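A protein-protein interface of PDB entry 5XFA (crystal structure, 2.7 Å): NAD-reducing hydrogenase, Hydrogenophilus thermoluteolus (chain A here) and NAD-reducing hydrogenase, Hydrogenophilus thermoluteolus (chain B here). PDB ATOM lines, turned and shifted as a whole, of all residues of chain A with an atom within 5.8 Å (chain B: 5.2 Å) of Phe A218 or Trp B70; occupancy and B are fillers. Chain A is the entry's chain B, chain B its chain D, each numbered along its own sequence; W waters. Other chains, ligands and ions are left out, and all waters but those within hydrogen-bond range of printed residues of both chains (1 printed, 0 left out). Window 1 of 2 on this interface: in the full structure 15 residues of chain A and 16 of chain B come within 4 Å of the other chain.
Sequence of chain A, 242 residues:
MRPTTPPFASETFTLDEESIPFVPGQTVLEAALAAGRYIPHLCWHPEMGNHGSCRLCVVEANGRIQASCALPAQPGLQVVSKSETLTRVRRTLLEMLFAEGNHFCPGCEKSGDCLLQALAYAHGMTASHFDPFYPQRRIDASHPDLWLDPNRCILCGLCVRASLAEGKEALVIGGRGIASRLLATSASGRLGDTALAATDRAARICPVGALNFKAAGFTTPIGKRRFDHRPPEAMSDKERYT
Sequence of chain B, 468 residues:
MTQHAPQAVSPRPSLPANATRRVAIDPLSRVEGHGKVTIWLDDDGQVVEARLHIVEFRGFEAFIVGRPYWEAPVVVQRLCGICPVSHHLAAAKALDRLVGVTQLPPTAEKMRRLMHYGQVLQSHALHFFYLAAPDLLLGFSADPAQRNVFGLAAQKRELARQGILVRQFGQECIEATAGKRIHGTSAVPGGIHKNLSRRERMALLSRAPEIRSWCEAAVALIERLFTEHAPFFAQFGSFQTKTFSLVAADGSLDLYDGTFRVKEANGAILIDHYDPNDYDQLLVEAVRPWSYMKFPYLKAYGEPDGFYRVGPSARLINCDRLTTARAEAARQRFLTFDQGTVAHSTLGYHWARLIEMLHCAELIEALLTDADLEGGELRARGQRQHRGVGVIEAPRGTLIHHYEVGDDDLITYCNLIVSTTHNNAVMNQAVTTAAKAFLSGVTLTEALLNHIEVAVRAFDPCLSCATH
Of the 13 printed residues of chain A, 9 touch a printed residue of chain B. Printed residues of chain A that touch a printed residue of chain B: Pro A106, Gly A107, Glu A109, Trp A147, Lys A214, Ala A215, Phe A218, Thr A219 and Thr A220. Of the 13 printed residues of chain B, 9 touch a printed residue of chain A. Hydrophobic or aromatic side chains of chain B within 4 Å of the printed part of chain A: Pro B68, Tyr B69, Trp B70, Val B74, Val B188 and His B193. Among the printed residues, 16 pairs touch across the chains. Among the printed residues, Asp or Glu carboxylates within 4 Å of a Lys or Arg side-chain nitrogen of the other chain: Lys A214 with Asp B409.
The side-chain carboxylate (OE1) of Glu A109 sits close to the indole nitrogen (NE1) of Trp A147, at 3.4 Å. N of Tyr B69 sits at hydrogen-bond distance from O of Asp B409 (3.0 Å).
Water W1 lies within hydrogen-bond range of OE2 of Glu B71 (2.7 Å) and N of Glu A109 (2.9 Å).
NE1 of Trp B70 sits at hydrogen-bond distance from OE1 of Glu A109 (3.2 Å). The side-chain carboxylate (OD1) of Asp B409 lies within salt-bridge range of the side-chain amino group (NZ) of Lys A214, at 3.9 Å. O of Phe A218 sits at hydrogen-bond distance from ND1 of His B193 (2.8 Å). The backbone carbonyl oxygen (O) of Gly A107 sits close to the side-chain carboxylate (OE2) of Glu B71.
Among the printed residues, merely in contact across the chains: Pro A106 with Val B74, Trp A147 with Pro B68, Trp A147 with Trp B70, Lys A214 with Trp B70, Ala A215 with Tyr B69, Ala A215 with Trp B70, Phe A218 with Trp B70, Phe A218 with Val B74, Phe A218 with Thr B185, Phe A218 with Val B188, Thr A219 with His B193 and Thr A220 with His B193.
Printed residues of chain B within 4 Å of Ala A215: Tyr B69 (3.6 Å) and Trp B70 (3.2 Å). Printed residues of chain B within 4 Å of Phe A218: Trp B70, Val B74, Thr B185, Val B188 and His B193. Pro B73 touches none of the printed residues of chain A. Of the printed residues of chain A, His B193 touches Phe A218 (2.8 Å), Thr A219 (3.8 Å) and Thr A220 (3.8 Å).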
ATOM      1  N   PRO A 106     -22.360  21.770 -14.052  1.00  0.00           N
ATOM      2  CA  PRO A 106     -21.276  20.904 -13.537  1.00  0.00           C
ATOM      3  C   PRO A 106     -19.851  21.150 -14.048  1.00  0.00           C
ATOM      4  O   PRO A 106     -18.895  20.650 -13.450  1.00  0.00           O
ATOM      5  CB  PRO A 106     -21.718  19.499 -13.957  1.00  0.00           C
ATOM      6  CG  PRO A 106     -23.193  19.581 -14.018  1.00  0.00           C
ATOM      7  CD  PRO A 106     -23.484  20.954 -14.547  1.00  0.00           C
ATOM      8  N   GLY A 107     -19.712  21.869 -15.149  1.00  0.00           N
ATOM      9  CA  GLY A 107     -18.399  22.223 -15.630  1.00  0.00           C
ATOM     10  C   GLY A 107     -18.248  23.694 -15.906  1.00  0.00           C
ATOM     11  O   GLY A 107     -17.337  24.068 -16.656  1.00  0.00           O
ATOM     12  N   CYS A 108     -19.164  24.506 -15.332  1.00  0.00           N
ATOM     13  CA  CYS A 108     -19.167  25.966 -15.438  1.00  0.00           C
ATOM     14  C   CYS A 108     -18.386  26.500 -14.284  1.00  0.00           C
ATOM     15  O   CYS A 108     -18.608  26.105 -13.123  1.00  0.00           O
ATOM     16  CB  CYS A 108     -20.562  26.543 -15.353  1.00  0.00           C
ATOM     17  SG  CYS A 108     -20.662  28.369 -15.458  1.00  0.00           S
ATOM     18  N   GLU A 109     -17.484  27.427 -14.589  1.00  0.00           N
ATOM     19  CA  GLU A 109     -16.603  27.959 -13.587  1.00  0.00           C
ATOM     20  C   GLU A 109     -17.318  29.055 -12.769  1.00  0.00           C
ATOM     21  O   GLU A 109     -16.731  29.551 -11.801  1.00  0.00           O
ATOM     22  CB  GLU A 109     -15.336  28.474 -14.255  1.00  0.00           C
ATOM     23  CG  GLU A 109     -15.475  29.879 -14.844  1.00  0.00           C
ATOM     24  CD  GLU A 109     -14.345  30.232 -15.787  1.00  0.00           C
ATOM     25  OE1 GLU A 109     -14.374  29.727 -16.930  1.00  0.00           O
ATOM     26  OE2 GLU A 109     -13.432  30.991 -15.377  1.00  0.00           O
ATOM     27  N   TRP A 147     -12.532  35.678 -21.870  1.00  0.00           N
ATOM     28  CA  TRP A 147     -13.170  34.791 -22.788  1.00  0.00           C
ATOM     29  C   TRP A 147     -14.636  34.809 -22.585  1.00  0.00           C
ATOM     30  O   TRP A 147     -15.093  35.087 -21.487  1.00  0.00           O
ATOM     31  CB  TRP A 147     -12.582  33.355 -22.652  1.00  0.00           C
ATOM     32  CG  TRP A 147     -13.056  32.568 -21.530  1.00  0.00           C
ATOM     33  CD1 TRP A 147     -12.682  32.687 -20.250  1.00  0.00           C
ATOM     34  CD2 TRP A 147     -13.991  31.495 -21.593  1.00  0.00           C
ATOM     35  NE1 TRP A 147     -13.338  31.761 -19.489  1.00  0.00           N
ATOM     36  CE2 TRP A 147     -14.151  31.012 -20.293  1.00  0.00           C
ATOM     37  CE3 TRP A 147     -14.692  30.875 -22.635  1.00  0.00           C
ATOM     38  CZ2 TRP A 147     -14.999  29.924 -19.981  1.00  0.00           C
ATOM     39  CZ3 TRP A 147     -15.559  29.810 -22.336  1.00  0.00           C
ATOM     40  CH2 TRP A 147     -15.697  29.343 -21.014  1.00  0.00           C
ATOM     41  N   PHE A 213     -12.914  36.312 -16.962  1.00  0.00           N
ATOM     42  CA  PHE A 213     -11.464  36.311 -16.935  1.00  0.00           C
ATOM     43  C   PHE A 213     -10.884  34.921 -17.355  1.00  0.00           C
ATOM     44  O   PHE A 213     -11.524  33.871 -17.177  1.00  0.00           O
ATOM     45  CB  PHE A 213     -10.946  36.689 -15.537  1.00  0.00           C
ATOM     46  CG  PHE A 213     -11.299  38.071 -15.133  1.00  0.00           C
ATOM     47  CD1 PHE A 213     -10.789  39.177 -15.858  1.00  0.00           C
ATOM     48  CD2 PHE A 213     -12.179  38.308 -14.096  1.00  0.00           C
ATOM     49  CE1 PHE A 213     -11.134  40.489 -15.527  1.00  0.00           C
ATOM     50  CE2 PHE A 213     -12.534  39.616 -13.761  1.00  0.00           C
ATOM     51  CZ  PHE A 213     -12.019  40.712 -14.486  1.00  0.00           C
ATOM     52  N   LYS A 214      -9.694  34.938 -17.946  1.00  0.00           N
ATOM     53  CA  LYS A 214      -9.035  33.727 -18.331  1.00  0.00           C
ATOM     54  C   LYS A 214      -8.196  33.240 -17.172  1.00  0.00           C
ATOM     55  O   LYS A 214      -7.545  34.048 -16.503  1.00  0.00           O
ATOM     56  CB  LYS A 214      -8.158  33.948 -19.554  1.00  0.00           C
ATOM     57  CG  LYS A 214      -8.892  33.811 -20.880  1.00  0.00           C
ATOM     58  CD  LYS A 214      -7.920  33.821 -22.048  1.00  0.00           C
ATOM     59  CE  LYS A 214      -8.654  33.688 -23.375  1.00  0.00           C
ATOM     60  NZ  LYS A 214      -7.827  34.228 -24.493  1.00  0.00           N
ATOM     61  N   ALA A 215      -8.266  31.921 -16.929  1.00  0.00           N
ATOM     62  CA  ALA A 215      -7.428  31.202 -15.974  1.00  0.00           C
ATOM     63  C   ALA A 215      -7.616  31.779 -14.580  1.00  0.00           C
ATOM     64  O   ALA A 215      -6.662  32.139 -13.887  1.00  0.00           O
ATOM     65  CB  ALA A 215      -5.963  31.235 -16.394  1.00  0.00           C
ATOM     66  N   ALA A 216      -8.867  31.856 -14.177  1.00  0.00           N
ATOM     67  CA  ALA A 216      -9.221  32.327 -12.860  1.00  0.00           C
ATOM     68  C   ALA A 216     -10.477  31.596 -12.487  1.00  0.00           C
ATOM     69  O   ALA A 216     -11.479  32.209 -12.147  1.00  0.00           O
ATOM     70  CB  ALA A 216      -9.481  33.811 -12.915  1.00  0.00           C
ATOM     71  N   GLY A 217     -10.425  30.277 -12.588  1.00  0.00           N
ATOM     72  CA  GLY A 217     -11.608  29.465 -12.470  1.00  0.00           C
ATOM     73  C   GLY A 217     -11.357  28.313 -11.548  1.00  0.00           C
ATOM     74  O   GLY A 217     -10.313  27.667 -11.615  1.00  0.00           O
ATOM     75  N   PHE A 218     -12.330  28.042 -10.691  1.00  0.00           N
ATOM     76  CA  PHE A 218     -12.218  26.961  -9.711  1.00  0.00           C
ATOM     77  C   PHE A 218     -11.167  27.258  -8.637  1.00  0.00           C
ATOM     78  O   PHE A 218     -10.416  26.369  -8.207  1.00  0.00           O
ATOM     79  CB  PHE A 218     -11.947  25.641 -10.428  1.00  0.00           C
ATOM     80  CG  PHE A 218     -13.015  25.277 -11.405  1.00  0.00           C
ATOM     81  CD1 PHE A 218     -14.309  25.035 -10.973  1.00  0.00           C
ATOM     82  CD2 PHE A 218     -12.737  25.165 -12.750  1.00  0.00           C
ATOM     83  CE1 PHE A 218     -15.302  24.697 -11.877  1.00  0.00           C
ATOM     84  CE2 PHE A 218     -13.730  24.830 -13.669  1.00  0.00           C
ATOM     85  CZ  PHE A 218     -15.016  24.603 -13.235  1.00  0.00           C
ATOM     86  N   THR A 219     -11.120  28.524  -8.230  1.00  0.00           N
ATOM     87  CA  THR A 219     -10.148  28.980  -7.250  1.00  0.00           C
ATOM     88  C   THR A 219     -10.796  28.994  -5.884  1.00  0.00           C
ATOM     89  O   THR A 219     -10.116  29.214  -4.879  1.00  0.00           O
ATOM     90  CB  THR A 219      -9.632  30.412  -7.585  1.00  0.00           C
ATOM     91  OG1 THR A 219     -10.655  31.398  -7.317  1.00  0.00           O
ATOM     92  CG2 THR A 219      -9.192  30.506  -9.060  1.00  0.00           C
ATOM     93  N   THR A 220     -12.109  28.799  -5.850  1.00  0.00           N
ATOM     94  CA  THR A 220     -12.838  28.900  -4.601  1.00  0.00           C
ATOM     95  C   THR A 220     -13.438  27.562  -4.193  1.00  0.00           C
ATOM     96  O   THR A 220     -14.230  26.971  -4.932  1.00  0.00           O
ATOM     97  CB  THR A 220     -13.959  29.935  -4.702  1.00  0.00           C
ATOM     98  OG1 THR A 220     -13.423  31.165  -5.176  1.00  0.00           O
ATOM     99  CG2 THR A 220     -14.601  30.159  -3.338  1.00  0.00           C
ATOM    100  N   PRO B  68     -11.867  25.735 -22.530  1.00  0.00           N
ATOM    101  CA  PRO B  68     -10.662  26.232 -21.883  1.00  0.00           C
ATOM    102  C   PRO B  68      -9.980  25.156 -21.109  1.00  0.00           C
ATOM    103  O   PRO B  68     -10.650  24.257 -20.579  1.00  0.00           O
ATOM    104  CB  PRO B  68     -11.177  27.305 -20.930  1.00  0.00           C
ATOM    105  CG  PRO B  68     -12.617  26.991 -20.729  1.00  0.00           C
ATOM    106  CD  PRO B  68     -13.068  26.442 -22.045  1.00  0.00           C
ATOM    107  N   TYR B  69      -8.658  25.253 -21.006  1.00  0.00           N
ATOM    108  CA  TYR B  69      -7.893  24.208 -20.334  1.00  0.00           C
ATOM    109  C   TYR B  69      -8.326  23.963 -18.886  1.00  0.00           C
ATOM    110  O   TYR B  69      -8.418  22.810 -18.458  1.00  0.00           O
ATOM    111  CB  TYR B  69      -6.374  24.419 -20.466  1.00  0.00           C
ATOM    112  CG  TYR B  69      -5.718  25.516 -19.649  1.00  0.00           C
ATOM    113  CD1 TYR B  69      -5.313  25.295 -18.341  1.00  0.00           C
ATOM    114  CD2 TYR B  69      -5.417  26.740 -20.221  1.00  0.00           C
ATOM    115  CE1 TYR B  69      -4.694  26.290 -17.605  1.00  0.00           C
ATOM    116  CE2 TYR B  69      -4.804  27.738 -19.496  1.00  0.00           C
ATOM    117  CZ  TYR B  69      -4.437  27.513 -18.196  1.00  0.00           C
ATOM    118  OH  TYR B  69      -3.804  28.515 -17.486  1.00  0.00           O
ATOM    119  N   TRP B  70      -8.613  25.030 -18.142  1.00  0.00           N
ATOM    120  CA  TRP B  70      -8.936  24.892 -16.710  1.00  0.00           C
ATOM    121  C   TRP B  70     -10.244  24.139 -16.440  1.00  0.00           C
ATOM    122  O   TRP B  70     -10.487  23.713 -15.311  1.00  0.00           O
ATOM    123  CB  TRP B  70      -8.947  26.238 -16.000  1.00  0.00           C
ATOM    124  CG  TRP B  70      -9.773  27.260 -16.700  1.00  0.00           C
ATOM    125  CD1 TRP B  70     -11.100  27.449 -16.561  1.00  0.00           C
ATOM    126  CD2 TRP B  70      -9.325  28.208 -17.658  1.00  0.00           C
ATOM    127  NE1 TRP B  70     -11.516  28.438 -17.381  1.00  0.00           N
ATOM    128  CE2 TRP B  70     -10.440  28.931 -18.064  1.00  0.00           C
ATOM    129  CE3 TRP B  70      -8.088  28.507 -18.209  1.00  0.00           C
ATOM    130  CZ2 TRP B  70     -10.368  29.950 -18.996  1.00  0.00           C
ATOM    131  CZ3 TRP B  70      -8.009  29.505 -19.140  1.00  0.00           C
ATOM    132  CH2 TRP B  70      -9.147  30.222 -19.528  1.00  0.00           C
ATOM    133  N   GLU B  71     -11.060  23.928 -17.468  1.00  0.00           N
ATOM    134  CA  GLU B  71     -12.258  23.109 -17.314  1.00  0.00           C
ATOM    135  C   GLU B  71     -11.952  21.615 -17.174  1.00  0.00           C
ATOM    136  O   GLU B  71     -12.709  20.899 -16.548  1.00  0.00           O
ATOM    137  CB  GLU B  71     -13.250  23.359 -18.457  1.00  0.00           C
ATOM    138  CG  GLU B  71     -14.252  24.471 -18.141  1.00  0.00           C
ATOM    139  CD  GLU B  71     -15.321  24.655 -19.212  1.00  0.00           C
ATOM    140  OE1 GLU B  71     -15.393  23.806 -20.137  1.00  0.00           O
ATOM    141  OE2 GLU B  71     -16.066  25.682 -19.163  1.00  0.00           O
ATOM    142  N   ALA B  72     -10.839  21.154 -17.740  1.00  0.00           N
ATOM    143  CA  ALA B  72     -10.583  19.727 -17.919  1.00  0.00           C
ATOM    144  C   ALA B  72     -10.599  18.865 -16.648  1.00  0.00           C
ATOM    145  O   ALA B  72     -11.204  17.798 -16.627  1.00  0.00           O
ATOM    146  CB  ALA B  72      -9.261  19.548 -18.627  1.00  0.00           C
ATOM    147  N   PRO B  73      -9.900  19.295 -15.595  1.00  0.00           N
ATOM    148  CA  PRO B  73      -9.972  18.499 -14.388  1.00  0.00           C
ATOM    149  C   PRO B  73     -11.394  18.330 -13.868  1.00  0.00           C
ATOM    150  O   PRO B  73     -11.711  17.300 -13.254  1.00  0.00           O
ATOM    151  CB  PRO B  73      -9.122  19.311 -13.387  1.00  0.00           C
ATOM    152  CG  PRO B  73      -8.271  20.200 -14.222  1.00  0.00           C
ATOM    153  CD  PRO B  73      -9.185  20.564 -15.350  1.00  0.00           C
ATOM    154  N   VAL B  74     -12.232  19.336 -14.099  1.00  0.00           N
ATOM    155  CA  VAL B  74     -13.604  19.323 -13.630  1.00  0.00           C
ATOM    156  C   VAL B  74     -14.576  18.614 -14.580  1.00  0.00           C
ATOM    157  O   VAL B  74     -15.373  17.798 -14.127  1.00  0.00           O
ATOM    158  CB  VAL B  74     -14.068  20.754 -13.318  1.00  0.00           C
ATOM    159  CG1 VAL B  74     -15.552  20.785 -12.974  1.00  0.00           C
ATOM    160  CG2 VAL B  74     -13.237  21.292 -12.158  1.00  0.00           C
ATOM    161  N   LEU B  95      -1.996  19.403 -16.580  1.00  0.00           N
ATOM    162  CA  LEU B  95      -2.032  20.842 -16.713  1.00  0.00           C
ATOM    163  C   LEU B  95      -0.964  21.486 -15.854  1.00  0.00           C
ATOM    164  O   LEU B  95      -0.576  22.621 -16.133  1.00  0.00           O
ATOM    165  CB  LEU B  95      -3.409  21.418 -16.373  1.00  0.00           C
ATOM    166  CG  LEU B  95      -4.570  20.842 -17.181  1.00  0.00           C
ATOM    167  CD1 LEU B  95      -5.885  21.384 -16.664  1.00  0.00           C
ATOM    168  CD2 LEU B  95      -4.431  21.127 -18.658  1.00  0.00           C
ATOM    169  N   THR B 185     -13.271  19.815  -7.126  1.00  0.00           N
ATOM    170  CA  THR B 185     -12.714  20.890  -7.943  1.00  0.00           C
ATOM    171  C   THR B 185     -11.354  21.424  -7.465  1.00  0.00           C
ATOM    172  O   THR B 185     -10.831  22.410  -8.028  1.00  0.00           O
ATOM    173  CB  THR B 185     -13.701  22.098  -7.990  1.00  0.00           C
ATOM    174  OG1 THR B 185     -14.031  22.523  -6.659  1.00  0.00           O
ATOM    175  CG2 THR B 185     -14.990  21.714  -8.720  1.00  0.00           C
ATOM    176  N   VAL B 188      -5.930  21.844  -9.048  1.00  0.00           N
ATOM    177  CA  VAL B 188      -5.848  22.884 -10.116  1.00  0.00           C
ATOM    178  C   VAL B 188      -4.438  22.943 -10.723  1.00  0.00           C
ATOM    179  O   VAL B 188      -3.486  22.449 -10.119  1.00  0.00           O
ATOM    180  CB  VAL B 188      -6.279  24.303  -9.617  1.00  0.00           C
ATOM    181  CG1 VAL B 188      -7.762  24.331  -9.312  1.00  0.00           C
ATOM    182  CG2 VAL B 188      -5.505  24.736  -8.383  1.00  0.00           C
ATOM    183  N   PRO B 189      -4.295  23.541 -11.921  1.00  0.00           N
ATOM    184  CA  PRO B 189      -2.954  23.626 -12.493  1.00  0.00           C
ATOM    185  C   PRO B 189      -2.025  24.378 -11.556  1.00  0.00           C
ATOM    186  O   PRO B 189      -2.287  25.518 -11.219  1.00  0.00           O
ATOM    187  CB  PRO B 189      -3.176  24.412 -13.779  1.00  0.00           C
ATOM    188  CG  PRO B 189      -4.592  24.150 -14.127  1.00  0.00           C
ATOM    189  CD  PRO B 189      -5.307  24.102 -12.823  1.00  0.00           C
ATOM    190  N   HIS B 193      -6.519  24.201  -4.439  1.00  0.00           N
ATOM    191  CA  HIS B 193      -7.144  25.493  -4.075  1.00  0.00           C
ATOM    192  C   HIS B 193      -7.557  25.616  -2.608  1.00  0.00           C
ATOM    193  O   HIS B 193      -8.222  26.571  -2.233  1.00  0.00           O
ATOM    194  CB  HIS B 193      -8.306  25.868  -5.021  1.00  0.00           C
ATOM    195  CG  HIS B 193      -9.559  25.070  -4.844  1.00  0.00           C
ATOM    196  ND1 HIS B 193     -10.572  25.079  -5.778  1.00  0.00           N
ATOM    197  CD2 HIS B 193      -9.981  24.265  -3.844  1.00  0.00           C
ATOM    198  CE1 HIS B 193     -11.560  24.306  -5.368  1.00  0.00           C
ATOM    199  NE2 HIS B 193     -11.226  23.797  -4.196  1.00  0.00           N
ATOM    200  N   ASP B 409      -5.830  29.533 -25.079  1.00  0.00           N
ATOM    201  CA  ASP B 409      -6.116  28.858 -23.810  1.00  0.00           C
ATOM    202  C   ASP B 409      -7.208  27.812 -23.981  1.00  0.00           C
ATOM    203  O   ASP B 409      -7.631  27.224 -22.993  1.00  0.00           O
ATOM    204  CB  ASP B 409      -6.438  29.812 -22.665  1.00  0.00           C
ATOM    205  CG  ASP B 409      -5.295  30.778 -22.359  1.00  0.00           C
ATOM    206  OD1 ASP B 409      -5.188  31.835 -23.029  1.00  0.00           O
ATOM    207  OD2 ASP B 409      -4.520  30.503 -21.428  1.00  0.00           O
HETATM  208  O   HOH W   1     -16.451  27.599 -17.300  1.00  0.00           O
